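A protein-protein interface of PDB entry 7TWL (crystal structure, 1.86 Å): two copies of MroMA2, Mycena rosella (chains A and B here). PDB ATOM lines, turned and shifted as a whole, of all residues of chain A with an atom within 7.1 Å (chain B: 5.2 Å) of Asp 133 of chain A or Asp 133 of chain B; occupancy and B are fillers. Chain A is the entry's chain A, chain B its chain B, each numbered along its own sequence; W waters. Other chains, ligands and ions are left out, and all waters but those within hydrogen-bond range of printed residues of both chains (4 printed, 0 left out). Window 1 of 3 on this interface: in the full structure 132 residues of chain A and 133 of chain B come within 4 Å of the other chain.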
ATOM      1  N   ILE A  19     -25.233  14.522  16.876  1.00  0.00           N
ATOM      2  CA  ILE A  19     -25.354  13.731  18.095  1.00  0.00           C
ATOM      3  C   ILE A  19     -25.068  14.597  19.319  1.00  0.00           C
ATOM      4  O   ILE A  19     -25.842  14.586  20.290  1.00  0.00           O
ATOM      5  CB  ILE A  19     -24.470  12.462  18.062  1.00  0.00           C
ATOM      6  CG1 ILE A  19     -24.764  11.556  16.861  1.00  0.00           C
ATOM      7  CG2 ILE A  19     -24.577  11.702  19.381  1.00  0.00           C
ATOM      8  CD1 ILE A  19     -26.153  10.897  16.896  1.00  0.00           C
ATOM      9  N   HIS A  24     -22.971  19.892  16.790  1.00  0.00           N
ATOM     10  CA  HIS A  24     -22.906  19.085  15.581  1.00  0.00           C
ATOM     11  C   HIS A  24     -23.803  19.635  14.465  1.00  0.00           C
ATOM     12  O   HIS A  24     -23.773  19.108  13.357  1.00  0.00           O
ATOM     13  CB  HIS A  24     -23.199  17.607  15.864  1.00  0.00           C
ATOM     14  CG  HIS A  24     -22.058  16.845  16.461  1.00  0.00           C
ATOM     15  ND1 HIS A  24     -22.182  15.509  16.804  1.00  0.00           N
ATOM     16  CD2 HIS A  24     -20.795  17.217  16.798  1.00  0.00           C
ATOM     17  CE1 HIS A  24     -21.034  15.067  17.284  1.00  0.00           C
ATOM     18  NE2 HIS A  24     -20.167  16.107  17.309  1.00  0.00           N
ATOM     19  N   HIS A 101     -27.932  11.990  11.718  1.00  0.00           N
ATOM     20  CA  HIS A 101     -28.265  12.131  10.307  1.00  0.00           C
ATOM     21  C   HIS A 101     -29.726  11.697  10.134  1.00  0.00           C
ATOM     22  O   HIS A 101     -30.097  10.617  10.604  1.00  0.00           O
ATOM     23  CB  HIS A 101     -27.350  11.187   9.529  1.00  0.00           C
ATOM     24  CG  HIS A 101     -27.422  11.285   8.041  1.00  0.00           C
ATOM     25  ND1 HIS A 101     -28.603  11.116   7.336  1.00  0.00           N
ATOM     26  CD2 HIS A 101     -26.435  11.423   7.124  1.00  0.00           C
ATOM     27  CE1 HIS A 101     -28.350  11.210   6.043  1.00  0.00           C
ATOM     28  NE2 HIS A 101     -27.008  11.393   5.888  1.00  0.00           N
ATOM     29  N   VAL A 104     -30.333   8.045   8.546  1.00  0.00           N
ATOM     30  CA  VAL A 104     -29.562   6.909   9.030  1.00  0.00           C
ATOM     31  C   VAL A 104     -30.320   6.327  10.225  1.00  0.00           C
ATOM     32  O   VAL A 104     -30.386   6.959  11.282  1.00  0.00           O
ATOM     33  CB  VAL A 104     -28.112   7.347   9.358  1.00  0.00           C
ATOM     34  CG1 VAL A 104     -27.285   6.279  10.064  1.00  0.00           C
ATOM     35  CG2 VAL A 104     -27.383   7.790   8.089  1.00  0.00           C
ATOM     36  N   MET A 125     -33.534  15.887   1.433  1.00  0.00           N
ATOM     37  CA  MET A 125     -32.912  15.535   2.711  1.00  0.00           C
ATOM     38  C   MET A 125     -31.527  16.179   2.771  1.00  0.00           C
ATOM     39  O   MET A 125     -30.819  16.195   1.765  1.00  0.00           O
ATOM     40  CB  MET A 125     -32.755  14.014   2.866  1.00  0.00           C
ATOM     41  CG  MET A 125     -32.222  13.577   4.233  1.00  0.00           C
ATOM     42  SD  MET A 125     -32.138  11.789   4.395  1.00  0.00           S
ATOM     43  CE  MET A 125     -33.865  11.370   4.637  1.00  0.00           C
ATOM     44  N   LEU A 126     -31.158  16.720   3.939  1.00  0.00           N
ATOM     45  CA  LEU A 126     -29.795  17.189   4.158  1.00  0.00           C
ATOM     46  C   LEU A 126     -29.089  16.196   5.076  1.00  0.00           C
ATOM     47  O   LEU A 126     -29.701  15.683   6.014  1.00  0.00           O
ATOM     48  CB  LEU A 126     -29.799  18.571   4.820  1.00  0.00           C
ATOM     49  CG  LEU A 126     -30.586  19.684   4.124  1.00  0.00           C
ATOM     50  CD1 LEU A 126     -30.331  21.002   4.827  1.00  0.00           C
ATOM     51  CD2 LEU A 126     -30.201  19.796   2.660  1.00  0.00           C
ATOM     52  N   PRO A 127     -27.772  15.933   4.881  1.00  0.00           N
ATOM     53  CA  PRO A 127     -27.045  15.017   5.760  1.00  0.00           C
ATOM     54  C   PRO A 127     -26.812  15.704   7.106  1.00  0.00           C
ATOM     55  O   PRO A 127     -26.806  16.930   7.207  1.00  0.00           O
ATOM     56  CB  PRO A 127     -25.702  14.807   5.036  1.00  0.00           C
ATOM     57  CG  PRO A 127     -25.507  16.088   4.232  1.00  0.00           C
ATOM     58  CD  PRO A 127     -26.914  16.549   3.857  1.00  0.00           C
ATOM     59  N   GLY A 128     -26.641  14.879   8.138  1.00  0.00           N
ATOM     60  CA  GLY A 128     -26.211  15.355   9.443  1.00  0.00           C
ATOM     61  C   GLY A 128     -25.127  14.427   9.972  1.00  0.00           C
ATOM     62  O   GLY A 128     -24.828  13.427   9.327  1.00  0.00           O
ATOM     63  N   ILE A 129     -24.600  14.730  11.165  1.00  0.00           N
ATOM     64  CA  ILE A 129     -23.547  13.936  11.785  1.00  0.00           C
ATOM     65  C   ILE A 129     -24.184  12.716  12.437  1.00  0.00           C
ATOM     66  O   ILE A 129     -24.979  12.877  13.361  1.00  0.00           O
ATOM     67  CB  ILE A 129     -22.808  14.774  12.852  1.00  0.00           C
ATOM     68  CG1 ILE A 129     -22.162  16.032  12.262  1.00  0.00           C
ATOM     69  CG2 ILE A 129     -21.817  13.890  13.609  1.00  0.00           C
ATOM     70  CD1 ILE A 129     -20.986  15.731  11.305  1.00  0.00           C
ATOM     71  N   SER A 130     -23.795  11.514  11.984  1.00  0.00           N
ATOM     72  CA  SER A 130     -24.363  10.275  12.494  1.00  0.00           C
ATOM     73  C   SER A 130     -23.593   9.775  13.721  1.00  0.00           C
ATOM     74  O   SER A 130     -22.470  10.206  13.996  1.00  0.00           O
ATOM     75  CB  SER A 130     -24.388   9.216  11.404  1.00  0.00           C
ATOM     76  OG  SER A 130     -23.131   8.550  11.299  1.00  0.00           O
ATOM     77  N   ALA A 131     -24.179   8.806  14.427  1.00  0.00           N
ATOM     78  CA  ALA A 131     -23.483   8.112  15.507  1.00  0.00           C
ATOM     79  C   ALA A 131     -22.227   7.407  14.996  1.00  0.00           C
ATOM     80  O   ALA A 131     -21.243   7.329  15.719  1.00  0.00           O
ATOM     81  CB  ALA A 131     -24.400   7.118  16.185  1.00  0.00           C
ATOM     82  N   GLU A 132     -22.264   6.866  13.765  1.00  0.00           N
ATOM     83  CA  GLU A 132     -21.066   6.272  13.170  1.00  0.00           C
ATOM     84  C   GLU A 132     -19.980   7.320  12.917  1.00  0.00           C
ATOM     85  O   GLU A 132     -18.802   7.064  13.168  1.00  0.00           O
ATOM     86  CB  GLU A 132     -21.411   5.514  11.884  1.00  0.00           C
ATOM     87  CG  GLU A 132     -21.329   4.023  12.077  1.00  0.00           C
ATOM     88  CD  GLU A 132     -21.651   3.254  10.808  1.00  0.00           C
ATOM     89  OE1 GLU A 132     -21.417   3.806   9.700  1.00  0.00           O
ATOM     90  OE2 GLU A 132     -22.129   2.116  10.934  1.00  0.00           O
ATOM     91  N   ASP A 133     -20.361   8.512  12.427  1.00  0.00           N
ATOM     92  CA  ASP A 133     -19.390   9.596  12.273  1.00  0.00           C
ATOM     93  C   ASP A 133     -18.722   9.915  13.617  1.00  0.00           C
ATOM     94  O   ASP A 133     -17.504  10.096  13.700  1.00  0.00           O
ATOM     95  CB  ASP A 133     -20.053  10.873  11.743  1.00  0.00           C
ATOM     96  CG  ASP A 133     -20.503  10.789  10.293  1.00  0.00           C
ATOM     97  OD1 ASP A 133     -19.845  10.062   9.520  1.00  0.00           O
ATOM     98  OD2 ASP A 133     -21.493  11.487   9.938  1.00  0.00           O
ATOM     99  N   TYR A 134     -19.535  10.012  14.672  1.00  0.00           N
ATOM    100  CA  TYR A 134     -19.038  10.300  16.014  1.00  0.00           C
ATOM    101  C   TYR A 134     -18.084   9.189  16.446  1.00  0.00           C
ATOM    102  O   TYR A 134     -17.013   9.459  16.991  1.00  0.00           O
ATOM    103  CB  TYR A 134     -20.233  10.474  16.962  1.00  0.00           C
ATOM    104  CG  TYR A 134     -20.094  11.441  18.115  1.00  0.00           C
ATOM    105  CD1 TYR A 134     -18.935  12.185  18.337  1.00  0.00           C
ATOM    106  CD2 TYR A 134     -21.148  11.616  19.005  1.00  0.00           C
ATOM    107  CE1 TYR A 134     -18.835  13.072  19.404  1.00  0.00           C
ATOM    108  CE2 TYR A 134     -21.063  12.503  20.072  1.00  0.00           C
ATOM    109  CZ  TYR A 134     -19.903  13.230  20.277  1.00  0.00           C
ATOM    110  OH  TYR A 134     -19.827  14.115  21.328  1.00  0.00           O
ATOM    111  N   MET A 135     -18.473   7.932  16.169  1.00  0.00           N
ATOM    112  CA  MET A 135     -17.678   6.774  16.525  1.00  0.00           C
ATOM    113  C   MET A 135     -16.284   6.818  15.881  1.00  0.00           C
ATOM    114  O   MET A 135     -15.285   6.565  16.561  1.00  0.00           O
ATOM    115  CB  MET A 135     -18.384   5.475  16.106  1.00  0.00           C
ATOM    116  CG  MET A 135     -17.551   4.258  16.443  1.00  0.00           C
ATOM    117  SD  MET A 135     -18.281   2.679  15.944  1.00  0.00           S
ATOM    118  CE  MET A 135     -19.338   2.380  17.364  1.00  0.00           C
ATOM    119  N   PHE A 136     -16.202   7.106  14.571  1.00  0.00           N
ATOM    120  CA  PHE A 136     -14.893   7.073  13.912  1.00  0.00           C
ATOM    121  C   PHE A 136     -13.957   8.093  14.563  1.00  0.00           C
ATOM    122  O   PHE A 136     -12.759   7.830  14.738  1.00  0.00           O
ATOM    123  CB  PHE A 136     -14.994   7.389  12.413  1.00  0.00           C
ATOM    124  CG  PHE A 136     -15.896   6.486  11.608  1.00  0.00           C
ATOM    125  CD1 PHE A 136     -15.853   5.105  11.769  1.00  0.00           C
ATOM    126  CD2 PHE A 136     -16.763   7.025  10.664  1.00  0.00           C
ATOM    127  CE1 PHE A 136     -16.676   4.283  11.007  1.00  0.00           C
ATOM    128  CE2 PHE A 136     -17.593   6.203   9.909  1.00  0.00           C
ATOM    129  CZ  PHE A 136     -17.544   4.832  10.081  1.00  0.00           C
ATOM    130  N   ALA A 137     -14.519   9.246  14.947  1.00  0.00           N
ATOM    131  CA  ALA A 137     -13.767  10.310  15.595  1.00  0.00           C
ATOM    132  C   ALA A 137     -13.329   9.913  17.009  1.00  0.00           C
ATOM    133  O   ALA A 137     -12.168  10.115  17.379  1.00  0.00           O
ATOM    134  CB  ALA A 137     -14.564  11.604  15.580  1.00  0.00           C
ATOM    135  N   ASP A 138     -14.257   9.360  17.797  1.00  0.00           N
ATOM    136  CA  ASP A 138     -14.024   9.077  19.216  1.00  0.00           C
ATOM    137  C   ASP A 138     -13.163   7.820  19.388  1.00  0.00           C
ATOM    138  O   ASP A 138     -12.287   7.767  20.249  1.00  0.00           O
ATOM    139  CB  ASP A 138     -15.359   8.906  19.957  1.00  0.00           C
ATOM    140  CG  ASP A 138     -16.049  10.208  20.325  1.00  0.00           C
ATOM    141  OD1 ASP A 138     -15.362  11.232  20.340  1.00  0.00           O
ATOM    142  OD2 ASP A 138     -17.291  10.190  20.580  1.00  0.00           O
ATOM    143  N   ILE A 170     -19.986  -2.553  12.846  1.00  0.00           N
ATOM    144  CA  ILE A 170     -20.681  -1.650  13.743  1.00  0.00           C
ATOM    145  C   ILE A 170     -22.109  -2.173  13.877  1.00  0.00           C
ATOM    146  O   ILE A 170     -22.766  -2.414  12.866  1.00  0.00           O
ATOM    147  CB  ILE A 170     -20.617  -0.197  13.223  1.00  0.00           C
ATOM    148  CG1 ILE A 170     -19.166   0.255  12.983  1.00  0.00           C
ATOM    149  CG2 ILE A 170     -21.325   0.725  14.201  1.00  0.00           C
ATOM    150  CD1 ILE A 170     -19.019   1.575  12.252  1.00  0.00           C
ATOM    151  N   TRP A 172     -25.784  -1.483  15.622  1.00  0.00           N
ATOM    152  CA  TRP A 172     -26.588  -0.403  16.164  1.00  0.00           C
ATOM    153  C   TRP A 172     -27.818  -0.988  16.864  1.00  0.00           C
ATOM    154  O   TRP A 172     -28.238  -2.112  16.560  1.00  0.00           O
ATOM    155  CB  TRP A 172     -27.066   0.550  15.053  1.00  0.00           C
ATOM    156  CG  TRP A 172     -26.077   1.253  14.161  1.00  0.00           C
ATOM    157  CD1 TRP A 172     -25.084   0.707  13.389  1.00  0.00           C
ATOM    158  CD2 TRP A 172     -26.056   2.663  13.883  1.00  0.00           C
ATOM    159  NE1 TRP A 172     -24.433   1.691  12.678  1.00  0.00           N
ATOM    160  CE2 TRP A 172     -25.009   2.897  12.960  1.00  0.00           C
ATOM    161  CE3 TRP A 172     -26.799   3.755  14.349  1.00  0.00           C
ATOM    162  CZ2 TRP A 172     -24.728   4.172  12.473  1.00  0.00           C
ATOM    163  CZ3 TRP A 172     -26.517   5.015  13.873  1.00  0.00           C
ATOM    164  CH2 TRP A 172     -25.474   5.220  12.961  1.00  0.00           C
ATOM    165  N   TYR A 209     -19.856   1.753  22.760  1.00  0.00           N
ATOM    166  CA  TYR A 209     -19.687   3.163  22.439  1.00  0.00           C
ATOM    167  C   TYR A 209     -20.963   3.946  22.710  1.00  0.00           C
ATOM    168  O   TYR A 209     -22.031   3.605  22.185  1.00  0.00           O
ATOM    169  CB  TYR A 209     -19.312   3.346  20.959  1.00  0.00           C
ATOM    170  CG  TYR A 209     -19.259   4.791  20.531  1.00  0.00           C
ATOM    171  CD1 TYR A 209     -18.384   5.675  21.148  1.00  0.00           C
ATOM    172  CD2 TYR A 209     -20.099   5.290  19.545  1.00  0.00           C
ATOM    173  CE1 TYR A 209     -18.327   7.012  20.774  1.00  0.00           C
ATOM    174  CE2 TYR A 209     -20.049   6.619  19.155  1.00  0.00           C
ATOM    175  CZ  TYR A 209     -19.136   7.475  19.752  1.00  0.00           C
ATOM    176  OH  TYR A 209     -19.121   8.791  19.400  1.00  0.00           O
ATOM    177  N   HIS B 101     -15.553  14.101   6.416  1.00  0.00           N
ATOM    178  CA  HIS B 101     -15.231  13.712   7.784  1.00  0.00           C
ATOM    179  C   HIS B 101     -13.720  13.479   7.818  1.00  0.00           C
ATOM    180  O   HIS B 101     -13.201  12.758   6.971  1.00  0.00           O
ATOM    181  CB  HIS B 101     -15.995  12.419   8.094  1.00  0.00           C
ATOM    182  CG  HIS B 101     -15.850  11.897   9.485  1.00  0.00           C
ATOM    183  ND1 HIS B 101     -14.610  11.645  10.069  1.00  0.00           N
ATOM    184  CD2 HIS B 101     -16.793  11.521  10.383  1.00  0.00           C
ATOM    185  CE1 HIS B 101     -14.799  11.175  11.300  1.00  0.00           C
ATOM    186  NE2 HIS B 101     -16.154  11.071  11.510  1.00  0.00           N
ATOM    187  N   VAL B 104     -12.521   9.634   7.825  1.00  0.00           N
ATOM    188  CA  VAL B 104     -13.121   8.691   6.887  1.00  0.00           C
ATOM    189  C   VAL B 104     -12.336   8.746   5.573  1.00  0.00           C
ATOM    190  O   VAL B 104     -12.388   9.754   4.868  1.00  0.00           O
ATOM    191  CB  VAL B 104     -14.626   9.016   6.714  1.00  0.00           C
ATOM    192  CG1 VAL B 104     -15.285   8.256   5.555  1.00  0.00           C
ATOM    193  CG2 VAL B 104     -15.386   8.773   8.016  1.00  0.00           C
ATOM    194  N   PRO B 127     -16.139  14.856  14.296  1.00  0.00           N
ATOM    195  CA  PRO B 127     -16.741  14.313  13.081  1.00  0.00           C
ATOM    196  C   PRO B 127     -17.108  15.420  12.096  1.00  0.00           C
ATOM    197  O   PRO B 127     -17.294  16.578  12.476  1.00  0.00           O
ATOM    198  CB  PRO B 127     -17.999  13.589  13.608  1.00  0.00           C
ATOM    199  CG  PRO B 127     -18.384  14.435  14.830  1.00  0.00           C
ATOM    200  CD  PRO B 127     -17.042  14.820  15.463  1.00  0.00           C
ATOM    201  N   GLY B 128     -17.175  15.044  10.814  1.00  0.00           N
ATOM    202  CA  GLY B 128     -17.732  15.930   9.805  1.00  0.00           C
ATOM    203  C   GLY B 128     -18.671  15.143   8.895  1.00  0.00           C
ATOM    204  O   GLY B 128     -18.770  13.924   9.040  1.00  0.00           O
ATOM    205  N   ILE B 129     -19.333  15.845   7.960  1.00  0.00           N
ATOM    206  CA  ILE B 129     -20.235  15.224   6.996  1.00  0.00           C
ATOM    207  C   ILE B 129     -19.424  14.500   5.917  1.00  0.00           C
ATOM    208  O   ILE B 129     -18.713  15.150   5.150  1.00  0.00           O
ATOM    209  CB  ILE B 129     -21.154  16.289   6.355  1.00  0.00           C
ATOM    210  CG1 ILE B 129     -21.962  17.076   7.394  1.00  0.00           C
ATOM    211  CG2 ILE B 129     -22.038  15.651   5.284  1.00  0.00           C
ATOM    212  CD1 ILE B 129     -23.037  16.248   8.094  1.00  0.00           C
ATOM    213  N   SER B 130     -19.584  13.170   5.826  1.00  0.00           N
ATOM    214  CA  SER B 130     -18.849  12.340   4.881  1.00  0.00           C
ATOM    215  C   SER B 130     -19.570  12.246   3.531  1.00  0.00           C
ATOM    216  O   SER B 130     -20.735  12.638   3.398  1.00  0.00           O
ATOM    217  CB  SER B 130     -18.605  10.964   5.457  1.00  0.00           C
ATOM    218  OG  SER B 130     -19.772  10.151   5.332  1.00  0.00           O
ATOM    219  N   ALA B 131     -18.869  11.692   2.531  1.00  0.00           N
ATOM    220  CA  ALA B 131     -19.500  11.438   1.244  1.00  0.00           C
ATOM    221  C   ALA B 131     -20.649  10.436   1.386  1.00  0.00           C
ATOM    222  O   ALA B 131     -21.634  10.553   0.664  1.00  0.00           O
ATOM    223  CB  ALA B 131     -18.496  11.002   0.201  1.00  0.00           C
ATOM    224  N   GLU B 132     -20.520   9.460   2.303  1.00  0.00           N
ATOM    225  CA  GLU B 132     -21.594   8.500   2.539  1.00  0.00           C
ATOM    226  C   GLU B 132     -22.816   9.192   3.131  1.00  0.00           C
ATOM    227  O   GLU B 132     -23.943   8.894   2.740  1.00  0.00           O
ATOM    228  CB  GLU B 132     -21.145   7.357   3.449  1.00  0.00           C
ATOM    229  CG  GLU B 132     -20.795   6.114   2.673  1.00  0.00           C
ATOM    230  CD  GLU B 132     -20.430   4.918   3.540  1.00  0.00           C
ATOM    231  OE1 GLU B 132     -20.814   4.902   4.734  1.00  0.00           O
ATOM    232  OE2 GLU B 132     -19.764   4.001   3.008  1.00  0.00           O
ATOM    233  N   ASP B 133     -22.587  10.093   4.097  1.00  0.00           N
ATOM    234  CA  ASP B 133     -23.652  10.913   4.662  1.00  0.00           C
ATOM    235  C   ASP B 133     -24.401  11.621   3.541  1.00  0.00           C
ATOM    236  O   ASP B 133     -25.634  11.588   3.504  1.00  0.00           O
ATOM    237  CB  ASP B 133     -23.118  11.965   5.637  1.00  0.00           C
ATOM    238  CG  ASP B 133     -22.669  11.390   6.973  1.00  0.00           C
ATOM    239  OD1 ASP B 133     -23.213  10.335   7.374  1.00  0.00           O
ATOM    240  OD2 ASP B 133     -21.774  12.011   7.604  1.00  0.00           O
ATOM    241  N   TYR B 134     -23.639  12.261   2.637  1.00  0.00           N
ATOM    242  CA  TYR B 134     -24.214  12.986   1.511  1.00  0.00           C
ATOM    243  C   TYR B 134     -25.040  12.028   0.652  1.00  0.00           C
ATOM    244  O   TYR B 134     -26.161  12.373   0.242  1.00  0.00           O
ATOM    245  CB  TYR B 134     -23.110  13.699   0.715  1.00  0.00           C
ATOM    246  CG  TYR B 134     -23.458  15.011   0.048  1.00  0.00           C
ATOM    247  CD1 TYR B 134     -24.717  15.599   0.141  1.00  0.00           C
ATOM    248  CD2 TYR B 134     -22.483  15.706  -0.650  1.00  0.00           C
ATOM    249  CE1 TYR B 134     -24.997  16.818  -0.474  1.00  0.00           C
ATOM    250  CE2 TYR B 134     -22.733  16.931  -1.247  1.00  0.00           C
ATOM    251  CZ  TYR B 134     -23.998  17.488  -1.172  1.00  0.00           C
ATOM    252  OH  TYR B 134     -24.202  18.703  -1.779  1.00  0.00           O
ATOM    253  N   MET B 135     -24.487  10.828   0.411  1.00  0.00           N
ATOM    254  CA  MET B 135     -25.113   9.818  -0.434  1.00  0.00           C
ATOM    255  C   MET B 135     -26.465   9.365   0.135  1.00  0.00           C
ATOM    256  O   MET B 135     -27.441   9.250  -0.607  1.00  0.00           O
ATOM    257  CB  MET B 135     -24.197   8.604  -0.631  1.00  0.00           C
ATOM    258  CG  MET B 135     -24.872   7.450  -1.389  1.00  0.00           C
ATOM    259  SD  MET B 135     -23.862   5.959  -1.513  1.00  0.00           S
ATOM    260  CE  MET B 135     -22.824   6.414  -2.906  1.00  0.00           C
ATOM    261  N   PHE B 136     -26.534   9.067   1.444  1.00  0.00           N
ATOM    262  CA  PHE B 136     -27.824   8.630   1.985  1.00  0.00           C
ATOM    263  C   PHE B 136     -28.919   9.665   1.730  1.00  0.00           C
ATOM    264  O   PHE B 136     -30.065   9.302   1.425  1.00  0.00           O
ATOM    265  CB  PHE B 136     -27.722   8.333   3.482  1.00  0.00           C
ATOM    266  CG  PHE B 136     -26.663   7.327   3.861  1.00  0.00           C
ATOM    267  CD1 PHE B 136     -26.474   6.176   3.113  1.00  0.00           C
ATOM    268  CD2 PHE B 136     -25.882   7.519   4.991  1.00  0.00           C
ATOM    269  CE1 PHE B 136     -25.538   5.222   3.491  1.00  0.00           C
ATOM    270  CE2 PHE B 136     -24.929   6.581   5.351  1.00  0.00           C
ATOM    271  CZ  PHE B 136     -24.748   5.439   4.600  1.00  0.00           C
ATOM    272  N   ALA B 137     -28.578  10.951   1.902  1.00  0.00           N
ATOM    273  CA  ALA B 137     -29.510  12.055   1.701  1.00  0.00           C
ATOM    274  C   ALA B 137     -29.872  12.213   0.220  1.00  0.00           C
ATOM    275  O   ALA B 137     -31.038  12.435  -0.110  1.00  0.00           O
ATOM    276  CB  ALA B 137     -28.943  13.343   2.275  1.00  0.00           C
HETATM  277  O   HOH W   1     -32.925  14.577  -1.110  1.00  0.00           O
HETATM  278  O   HOH W   2     -22.732   3.184   6.648  1.00  0.00           O
HETATM  279  O   HOH W   3     -22.857   7.966   8.723  1.00  0.00           O
HETATM  280  O   HOH W   4     -19.801   8.558   7.315  1.00  0.00           O
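Printed residues of chain A that touch a printed residue of chain B: His 24, His 101, Val 104, Met 125, Pro 127, Gly 128, Ile 129, Asp 133, Phe 136 and Ala 137.
Of the 13 printed residues of chain B, 8 touch a printed residue of chain A.
Hydrophobic or aromatic side chains of chain B that line the printed part of chain A: His 101, Val 104, Pro 127, Ile 129, Phe 136 and Ala 137.
Among the printed residues, 20 pairs touch across the chains.
Among the printed residues, no Asp or Glu carboxylate lies within 4 Å of a Lys or Arg side-chain nitrogen of the other chain.
A ring nitrogen (NE2) of His 101 of chain A sits at hydrogen-bond distance from the backbone carbonyl oxygen (O) of Asp 133 of chain B (2.8 Å).
A ring nitrogen (NE2) of His 101 of chain B lies within hydrogen-bond range of the backbone carbonyl oxygen (O) of Asp 133 of chain A.
The side-chain carboxylate (OD2) of Asp 133 of chain B sits close to the side-chain carboxylate (OD2) of Asp 133 of chain A, 2.4 Å away.
Among the printed residues, merely in contact across the chains: Gly 128 of chain A with Ile 129 of chain B (3.3 Å), Ile 129 of chain A with Gly 128 of chain B (3.4 Å), Met 125 of chain A with Ala 137 of chain B (3.5 Å), Val 104 of chain A with Phe 136 of chain B (3.5 Å), Phe 136 of chain A with Val 104 of chain B (3.5 Å), His 24 of chain A with Pro 127 of chain B (3.5 Å), Asp 133 of chain A with Pro 127 of chain B (3.5 Å), Pro 127 of chain A with Asp 133 of chain B (3.6 Å), Pro 127 of chain A with Ile 129 of chain B (3.7 Å), Ile 129 of chain A with Pro 127 of chain B (3.7 Å), Ile 129 of chain A with Ile 129 of chain B (3.7 Å), Asp 133 of chain A with Gly 128 of chain B (3.8 Å), Gly 128 of chain A with Asp 133 of chain B (3.8 Å), Ala 137 of chain A with Pro 127 of chain B (3.8 Å), Pro 127 of chain A with Ala 137 of chain B (3.9 Å), His 101 of chain A with Phe 136 of chain B (3.9 Å) and Phe 136 of chain A with His 101 of chain B (3.95 Å).
Water W4 lies within hydrogen-bond range of the side-chain hydroxyl of Ser 130 of chain B and the side-chain carboxylate of Asp 133 of chain A.
Water W3 lies within hydrogen-bond range of OG of Ser 130 of chain A (2.7 Å) and OD1 of Asp 133 of chain B (2.7 Å).
Water W1 lies within hydrogen-bond range of the backbone NH (N) of Met 125 of chain A (2.9 Å) and the backbone carbonyl oxygen (O) of Ala 137 of chain B (3.0 Å).
Water W2 bridges OE1 of Glu 132 of chain B (3.2 Å) and OE1 of Glu 132 of chain A (3.4 Å).
Printed residues of chain B within 4 Å of His 101 of chain A: Asp 133 and Phe 136.
Printed residues of chain B within 4 Å of Pro 127 of chain A: Ile 129 (3.7 Å), Asp 133 (3.6 Å) and Ala 137 (3.9 Å).
Of the printed residues of chain B, Ile 129 of chain A touches Pro 127 (3.7 Å), Gly 128 (3.4 Å) and Ile 129 (3.7 Å).
Of chain B, only His 101, Pro 127, Gly 128 and Asp 133 come within 4 Å of Asp 133 of chain A.
Met 135 of chain A touches none of the printed residues of chain B.
Of the printed residues of chain B, Ala 137 of chain A touches Pro 127.
Of the printed residues of chain A, Gly 128 of chain B touches Ile 129 and Asp 133.
Glu 132 of chain B touches none of the printed residues of chain A.
Of chain A, only His 101, Pro 127, Gly 128 and Asp 133 come within 4 Å of Asp 133 of chain B.
The nearest printed residue of chain A that does not touch Ile 129 of chain B is Asp 133 of chain A (4.9 Å).
N of Ile 19 of chain A is in hydrogen-bond range of ND1 of His 24 of chain A (3.2 Å).
N of His 101 of chain A is in hydrogen-bond range of O of Ile 129 of chain A.
OG of Ser 130 of chain A sits at hydrogen-bond distance from N of Asp 133 of chain A, 3.0 Å away.
N of Ser 130 of chain B sits at hydrogen-bond distance from OD2 of Asp 133 of chain B, at 3.0 Å.
His 101 of chain A touches Asp 133 of chain B, and with the chains exchanged Asp 133 of chain A touches His 101 of chain B.
His 101 of chain A touches Phe 136 of chain B, and with the chains exchanged Phe 136 of chain A touches His 101 of chain B.
Pro 127 of chain A touches Ala 137 of chain B, and with the chains exchanged Ala 137 of chain A touches Pro 127 of chain B.
Gly 128 of chain A touches Asp 133 of chain B, and with the chains exchanged Asp 133 of chain A touches Gly 128 of chain B.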
